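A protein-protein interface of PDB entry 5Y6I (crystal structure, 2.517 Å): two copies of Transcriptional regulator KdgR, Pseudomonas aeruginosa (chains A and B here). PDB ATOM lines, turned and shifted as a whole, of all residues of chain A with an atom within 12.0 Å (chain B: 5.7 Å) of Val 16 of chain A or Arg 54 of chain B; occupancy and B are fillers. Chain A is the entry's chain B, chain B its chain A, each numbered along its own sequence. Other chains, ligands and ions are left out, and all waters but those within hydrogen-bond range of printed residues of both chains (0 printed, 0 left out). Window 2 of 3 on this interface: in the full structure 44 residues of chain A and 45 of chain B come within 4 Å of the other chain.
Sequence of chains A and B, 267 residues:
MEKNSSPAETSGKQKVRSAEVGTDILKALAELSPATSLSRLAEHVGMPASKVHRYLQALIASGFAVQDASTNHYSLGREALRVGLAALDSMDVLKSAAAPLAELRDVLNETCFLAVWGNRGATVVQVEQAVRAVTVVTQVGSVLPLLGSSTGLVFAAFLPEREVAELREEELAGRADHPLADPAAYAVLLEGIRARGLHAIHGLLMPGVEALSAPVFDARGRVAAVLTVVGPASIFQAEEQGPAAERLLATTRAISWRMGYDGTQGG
Of chain B, only Ser 18 (3.8 Å), Arg 54 (3.7 Å), Tyr 55 (3.96 Å) and Ala 58 (3.8 Å) come within 4 Å of Val 16 of chain A.
Of the printed residues of chain B, Ser 18 of chain A touches Ser 18 (3.6 Å).
Printed residues of chain B within 4 Å of Ala 19 of chain A: Ser 18 (2.9 Å) and Tyr 55 (3.5 Å).
Of the printed residues of chain B, Glu 20 of chain A touches Ala 58.
Val 21 of chain A touches none of the printed residues of chain B.
Ser 18 of chain B touches just these residues of chain A: Val 16, Ser 18 and Ala 19.
No residue of chain A comes within 4 Å of Val 52 of chain B.
No residue of chain A comes within 4 Å of His 53 of chain B.
Of chain A, only Val 16 (3.7 Å) comes within 4 Å of Arg 54 of chain B.
Of the printed residues of chain A, Tyr 55 of chain B touches Val 16 (3.96 Å) and Ala 19 (3.5 Å).
The nearest printed residue of chain B that does not touch Val 16 of chain A is Gln 57 of chain B (5.7 Å).
The nearest residue of chain A that does not touch Arg 54 of chain B is Arg 17 of chain A (6.8 Å).
OG of Ser 18 of chain B lies within hydrogen-bond range of N of Ala 19 of chain A, 2.9 Å away.
The backbone carbonyl oxygen (O) of Ala 58 of chain B lies close to the side-chain carboxylate (OE1) of Glu 20 of chain A (3.3 Å).
Hydrophobic or aromatic side chains of chain A within 4 Å of the printed part of chain B: Val 16 and Ala 19.
Of the 11 printed residues of chain B, 4 touch a printed residue of chain A.
Printed residues of chain B that touch a printed residue of chain A: Ser 18, Arg 54, Tyr 55 and Ala 58.
O of Glu 20 of chain A lies within hydrogen-bond range of OG1 of Thr 23 of chain A.
Among the printed residues, merely in contact across the chains: Ala 19 of chain A with Tyr 55 of chain B (3.5 Å), Ser 18 of chain A with Ser 18 of chain B (3.6 Å), Val 16 of chain A with Arg 54 of chain B (3.7 Å), Val 16 of chain A with Ala 58 of chain B (3.8 Å), Val 16 of chain A with Ser 18 of chain B (3.8 Å) and Val 16 of chain A with Tyr 55 of chain B (3.96 Å).
Ser 18 of chain B touches its own counterpart, Ser 18 of chain A.
3 positions are printed for both chains.
Of the 8 pairs that touch across the chains among the printed residues, 1 has its exchanged pair printed and touching as well.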
ATOM      1  N   VAL A  16     -28.681 -12.930  16.953  1.00  0.00           N
ATOM      2  CA  VAL A  16     -27.937 -11.754  16.525  1.00  0.00           C
ATOM      3  C   VAL A  16     -28.819 -10.904  15.606  1.00  0.00           C
ATOM      4  O   VAL A  16     -28.707  -9.683  15.594  1.00  0.00           O
ATOM      5  CB  VAL A  16     -26.610 -12.150  15.832  1.00  0.00           C
ATOM      6  CG1 VAL A  16     -25.670 -10.948  15.719  1.00  0.00           C
ATOM      7  CG2 VAL A  16     -25.942 -13.300  16.568  1.00  0.00           C
ATOM      8  N   ARG A  17     -29.705 -11.543  14.838  1.00  0.00           N
ATOM      9  CA  ARG A  17     -30.640 -10.762  14.035  1.00  0.00           C
ATOM     10  C   ARG A  17     -31.796 -10.258  14.892  1.00  0.00           C
ATOM     11  O   ARG A  17     -32.093  -9.058  14.913  1.00  0.00           O
ATOM     12  CB  ARG A  17     -31.152 -11.576  12.830  1.00  0.00           C
ATOM     13  CG  ARG A  17     -32.202 -12.681  13.059  1.00  0.00           C
ATOM     14  CD  ARG A  17     -31.713 -13.799  13.996  1.00  0.00           C
ATOM     15  NE  ARG A  17     -30.446 -14.337  13.521  1.00  0.00           N
ATOM     16  CZ  ARG A  17     -29.577 -14.998  14.277  1.00  0.00           C
ATOM     17  NH1 ARG A  17     -28.452 -15.438  13.733  1.00  0.00           N
ATOM     18  NH2 ARG A  17     -29.825 -15.224  15.562  1.00  0.00           N
ATOM     19  N   SER A  18     -32.430 -11.155  15.638  1.00  0.00           N
ATOM     20  CA  SER A  18     -33.542 -10.791  16.498  1.00  0.00           C
ATOM     21  C   SER A  18     -33.075 -10.183  17.814  1.00  0.00           C
ATOM     22  O   SER A  18     -33.905  -9.720  18.608  1.00  0.00           O
ATOM     23  CB  SER A  18     -34.425 -12.024  16.742  1.00  0.00           C
ATOM     24  OG  SER A  18     -34.673 -12.719  15.521  1.00  0.00           O
ATOM     25  N   ALA A  19     -31.763 -10.189  18.064  1.00  0.00           N
ATOM     26  CA  ALA A  19     -31.205  -9.380  19.141  1.00  0.00           C
ATOM     27  C   ALA A  19     -31.535  -7.913  18.938  1.00  0.00           C
ATOM     28  O   ALA A  19     -31.790  -7.188  19.908  1.00  0.00           O
ATOM     29  CB  ALA A  19     -29.690  -9.585  19.207  1.00  0.00           C
ATOM     30  N   GLU A  20     -31.563  -7.474  17.680  1.00  0.00           N
ATOM     31  CA  GLU A  20     -31.791  -6.080  17.342  1.00  0.00           C
ATOM     32  C   GLU A  20     -33.263  -5.718  17.247  1.00  0.00           C
ATOM     33  O   GLU A  20     -33.597  -4.542  17.399  1.00  0.00           O
ATOM     34  CB  GLU A  20     -31.106  -5.737  16.017  1.00  0.00           C
ATOM     35  CG  GLU A  20     -29.660  -6.160  15.947  1.00  0.00           C
ATOM     36  CD  GLU A  20     -28.984  -5.661  14.693  1.00  0.00           C
ATOM     37  OE1 GLU A  20     -28.326  -4.596  14.757  1.00  0.00           O
ATOM     38  OE2 GLU A  20     -29.111  -6.337  13.643  1.00  0.00           O
ATOM     39  N   VAL A  21     -34.155  -6.678  16.996  1.00  0.00           N
ATOM     40  CA  VAL A  21     -35.567  -6.314  17.054  1.00  0.00           C
ATOM     41  C   VAL A  21     -35.956  -6.021  18.489  1.00  0.00           C
ATOM     42  O   VAL A  21     -36.752  -5.109  18.745  1.00  0.00           O
ATOM     43  CB  VAL A  21     -36.474  -7.390  16.422  1.00  0.00           C
ATOM     44  CG1 VAL A  21     -36.193  -8.733  16.987  1.00  0.00           C
ATOM     45  CG2 VAL A  21     -37.941  -7.044  16.652  1.00  0.00           C
ATOM     46  N   GLY A  22     -35.375  -6.743  19.448  1.00  0.00           N
ATOM     47  CA  GLY A  22     -35.531  -6.380  20.845  1.00  0.00           C
ATOM     48  C   GLY A  22     -35.255  -4.911  21.086  1.00  0.00           C
ATOM     49  O   GLY A  22     -36.126  -4.174  21.557  1.00  0.00           O
ATOM     50  N   THR A  23     -34.045  -4.463  20.743  1.00  0.00           N
ATOM     51  CA  THR A  23     -33.702  -3.054  20.903  1.00  0.00           C
ATOM     52  C   THR A  23     -34.507  -2.159  19.966  1.00  0.00           C
ATOM     53  O   THR A  23     -34.745  -1.002  20.293  1.00  0.00           O
ATOM     54  CB  THR A  23     -32.197  -2.849  20.684  1.00  0.00           C
ATOM     55  OG1 THR A  23     -31.867  -3.063  19.302  1.00  0.00           O
ATOM     56  CG2 THR A  23     -31.371  -3.820  21.552  1.00  0.00           C
ATOM     57  N   ASP A  24     -34.960  -2.673  18.821  1.00  0.00           N
ATOM     58  CA  ASP A  24     -35.841  -1.886  17.963  1.00  0.00           C
ATOM     59  C   ASP A  24     -37.116  -1.508  18.698  1.00  0.00           C
ATOM     60  O   ASP A  24     -37.569  -0.357  18.629  1.00  0.00           O
ATOM     61  CB  ASP A  24     -36.178  -2.655  16.684  1.00  0.00           C
ATOM     62  CG  ASP A  24     -35.038  -2.657  15.680  1.00  0.00           C
ATOM     63  OD1 ASP A  24     -34.291  -1.657  15.610  1.00  0.00           O
ATOM     64  OD2 ASP A  24     -34.884  -3.661  14.944  1.00  0.00           O
ATOM     65  N   LYS A  51     -46.320 -10.537  17.836  1.00  0.00           N
ATOM     66  CA  LYS A  51     -44.862 -10.588  17.862  1.00  0.00           C
ATOM     67  C   LYS A  51     -44.301  -9.503  18.765  1.00  0.00           C
ATOM     68  O   LYS A  51     -43.395  -9.757  19.563  1.00  0.00           O
ATOM     69  CB  LYS A  51     -44.302 -10.456  16.445  1.00  0.00           C
ATOM     70  CG  LYS A  51     -42.794 -10.641  16.365  1.00  0.00           C
ATOM     71  CD  LYS A  51     -42.348 -10.889  14.936  1.00  0.00           C
ATOM     72  CE  LYS A  51     -40.858 -11.197  14.860  1.00  0.00           C
ATOM     73  NZ  LYS A  51     -40.435 -11.515  13.459  1.00  0.00           N
ATOM     74  N   TYR A  55     -41.861  -9.938  22.385  1.00  0.00           N
ATOM     75  CA  TYR A  55     -40.608  -9.221  22.639  1.00  0.00           C
ATOM     76  C   TYR A  55     -40.731  -8.269  23.826  1.00  0.00           C
ATOM     77  O   TYR A  55     -39.753  -8.054  24.554  1.00  0.00           O
ATOM     78  CB  TYR A  55     -40.151  -8.448  21.392  1.00  0.00           C
ATOM     79  CG  TYR A  55     -39.459  -9.313  20.347  1.00  0.00           C
ATOM     80  CD1 TYR A  55     -38.167  -9.785  20.554  1.00  0.00           C
ATOM     81  CD2 TYR A  55     -40.096  -9.651  19.158  1.00  0.00           C
ATOM     82  CE1 TYR A  55     -37.538 -10.579  19.621  1.00  0.00           C
ATOM     83  CE2 TYR A  55     -39.474 -10.442  18.216  1.00  0.00           C
ATOM     84  CZ  TYR A  55     -38.197 -10.908  18.450  1.00  0.00           C
ATOM     85  OH  TYR A  55     -37.580 -11.696  17.503  1.00  0.00           O
ATOM     86  N   SER B  18     -33.255 -14.432  22.045  1.00  0.00           N
ATOM     87  CA  SER B  18     -32.145 -13.531  21.758  1.00  0.00           C
ATOM     88  C   SER B  18     -32.406 -12.108  22.244  1.00  0.00           C
ATOM     89  O   SER B  18     -31.455 -11.359  22.498  1.00  0.00           O
ATOM     90  CB  SER B  18     -31.861 -13.542  20.257  1.00  0.00           C
ATOM     91  OG  SER B  18     -31.135 -12.397  19.857  1.00  0.00           O
ATOM     92  N   ALA B  49     -17.435 -15.781  26.427  1.00  0.00           N
ATOM     93  CA  ALA B  49     -16.935 -14.571  25.776  1.00  0.00           C
ATOM     94  C   ALA B  49     -17.349 -14.509  24.319  1.00  0.00           C
ATOM     95  O   ALA B  49     -17.612 -13.417  23.802  1.00  0.00           O
ATOM     96  CB  ALA B  49     -15.415 -14.483  25.874  1.00  0.00           C
ATOM     97  N   SER B  50     -17.444 -15.662  23.653  1.00  0.00           N
ATOM     98  CA  SER B  50     -17.743 -15.678  22.223  1.00  0.00           C
ATOM     99  C   SER B  50     -19.167 -15.207  21.943  1.00  0.00           C
ATOM    100  O   SER B  50     -19.392 -14.374  21.054  1.00  0.00           O
ATOM    101  CB  SER B  50     -17.485 -17.074  21.643  1.00  0.00           C
ATOM    102  OG  SER B  50     -17.922 -18.116  22.508  1.00  0.00           O
ATOM    103  N   LYS B  51     -20.150 -15.701  22.704  1.00  0.00           N
ATOM    104  CA  LYS B  51     -21.508 -15.201  22.513  1.00  0.00           C
ATOM    105  C   LYS B  51     -21.604 -13.712  22.832  1.00  0.00           C
ATOM    106  O   LYS B  51     -22.334 -12.982  22.152  1.00  0.00           O
ATOM    107  CB  LYS B  51     -22.503 -16.014  23.355  1.00  0.00           C
ATOM    108  CG  LYS B  51     -23.827 -15.326  23.634  1.00  0.00           C
ATOM    109  CD  LYS B  51     -24.884 -16.301  24.187  1.00  0.00           C
ATOM    110  CE  LYS B  51     -24.860 -16.362  25.714  1.00  0.00           C
ATOM    111  NZ  LYS B  51     -25.635 -17.480  26.346  1.00  0.00           N
ATOM    112  N   VAL B  52     -20.860 -13.226  23.829  1.00  0.00           N
ATOM    113  CA  VAL B  52     -20.914 -11.790  24.118  1.00  0.00           C
ATOM    114  C   VAL B  52     -20.376 -11.009  22.932  1.00  0.00           C
ATOM    115  O   VAL B  52     -21.012 -10.062  22.447  1.00  0.00           O
ATOM    116  CB  VAL B  52     -20.167 -11.446  25.425  1.00  0.00           C
ATOM    117  CG1 VAL B  52     -20.193  -9.925  25.695  1.00  0.00           C
ATOM    118  CG2 VAL B  52     -20.795 -12.177  26.593  1.00  0.00           C
ATOM    119  N   HIS B  53     -19.212 -11.415  22.421  1.00  0.00           N
ATOM    120  CA  HIS B  53     -18.661 -10.731  21.254  1.00  0.00           C
ATOM    121  C   HIS B  53     -19.646 -10.714  20.090  1.00  0.00           C
ATOM    122  O   HIS B  53     -19.747  -9.703  19.388  1.00  0.00           O
ATOM    123  CB  HIS B  53     -17.343 -11.364  20.806  1.00  0.00           C
ATOM    124  CG  HIS B  53     -16.883 -10.856  19.479  1.00  0.00           C
ATOM    125  ND1 HIS B  53     -16.125  -9.714  19.346  1.00  0.00           N
ATOM    126  CD2 HIS B  53     -17.139 -11.289  18.224  1.00  0.00           C
ATOM    127  CE1 HIS B  53     -15.911  -9.480  18.063  1.00  0.00           C
ATOM    128  NE2 HIS B  53     -16.514 -10.422  17.363  1.00  0.00           N
ATOM    129  N   ARG B  54     -20.390 -11.802  19.881  1.00  0.00           N
ATOM    130  CA  ARG B  54     -21.335 -11.847  18.770  1.00  0.00           C
ATOM    131  C   ARG B  54     -22.435 -10.814  18.948  1.00  0.00           C
ATOM    132  O   ARG B  54     -22.729 -10.044  18.025  1.00  0.00           O
ATOM    133  CB  ARG B  54     -21.932 -13.252  18.626  1.00  0.00           C
ATOM    134  CG  ARG B  54     -22.281 -13.585  17.183  1.00  0.00           C
ATOM    135  CD  ARG B  54     -22.511 -15.068  16.964  1.00  0.00           C
ATOM    136  NE  ARG B  54     -21.602 -15.915  17.735  1.00  0.00           N
ATOM    137  CZ  ARG B  54     -22.020 -16.871  18.561  1.00  0.00           C
ATOM    138  NH1 ARG B  54     -23.326 -17.078  18.706  1.00  0.00           N
ATOM    139  NH2 ARG B  54     -21.144 -17.615  19.235  1.00  0.00           N
ATOM    140  N   TYR B  55     -23.042 -10.770  20.142  1.00  0.00           N
ATOM    141  CA  TYR B  55     -24.130  -9.823  20.387  1.00  0.00           C
ATOM    142  C   TYR B  55     -23.617  -8.401  20.540  1.00  0.00           C
ATOM    143  O   TYR B  55     -24.345  -7.454  20.225  1.00  0.00           O
ATOM    144  CB  TYR B  55     -24.937 -10.225  21.623  1.00  0.00           C
ATOM    145  CG  TYR B  55     -25.867 -11.396  21.405  1.00  0.00           C
ATOM    146  CD1 TYR B  55     -25.424 -12.698  21.593  1.00  0.00           C
ATOM    147  CD2 TYR B  55     -27.186 -11.198  21.011  1.00  0.00           C
ATOM    148  CE1 TYR B  55     -26.260 -13.769  21.392  1.00  0.00           C
ATOM    149  CE2 TYR B  55     -28.030 -12.265  20.798  1.00  0.00           C
ATOM    150  CZ  TYR B  55     -27.562 -13.552  20.995  1.00  0.00           C
ATOM    151  OH  TYR B  55     -28.393 -14.634  20.800  1.00  0.00           O
ATOM    152  N   LEU B  56     -22.384  -8.227  21.029  1.00  0.00           N
ATOM    153  CA  LEU B  56     -21.763  -6.903  21.016  1.00  0.00           C
ATOM    154  C   LEU B  56     -21.818  -6.300  19.615  1.00  0.00           C
ATOM    155  O   LEU B  56     -22.288  -5.171  19.432  1.00  0.00           O
ATOM    156  CB  LEU B  56     -20.316  -6.978  21.523  1.00  0.00           C
ATOM    157  CG  LEU B  56     -20.093  -6.618  23.003  1.00  0.00           C
ATOM    158  CD1 LEU B  56     -18.645  -6.824  23.452  1.00  0.00           C
ATOM    159  CD2 LEU B  56     -20.526  -5.170  23.298  1.00  0.00           C
ATOM    160  N   GLN B  57     -21.395  -7.071  18.607  1.00  0.00           N
ATOM    161  CA  GLN B  57     -21.422  -6.598  17.224  1.00  0.00           C
ATOM    162  C   GLN B  57     -22.794  -6.038  16.849  1.00  0.00           C
ATOM    163  O   GLN B  57     -22.893  -4.932  16.302  1.00  0.00           O
ATOM    164  CB  GLN B  57     -21.021  -7.730  16.276  1.00  0.00           C
ATOM    165  CG  GLN B  57     -19.632  -8.297  16.546  1.00  0.00           C
ATOM    166  CD  GLN B  57     -18.573  -7.223  16.671  1.00  0.00           C
ATOM    167  OE1 GLN B  57     -18.094  -6.928  17.769  1.00  0.00           O
ATOM    168  NE2 GLN B  57     -18.198  -6.632  15.542  1.00  0.00           N
ATOM    169  N   ALA B  58     -23.867  -6.773  17.157  1.00  0.00           N
ATOM    170  CA  ALA B  58     -25.213  -6.270  16.877  1.00  0.00           C
ATOM    171  C   ALA B  58     -25.476  -4.951  17.604  1.00  0.00           C
ATOM    172  O   ALA B  58     -25.982  -3.991  17.008  1.00  0.00           O
ATOM    173  CB  ALA B  58     -26.262  -7.309  17.275  1.00  0.00           C
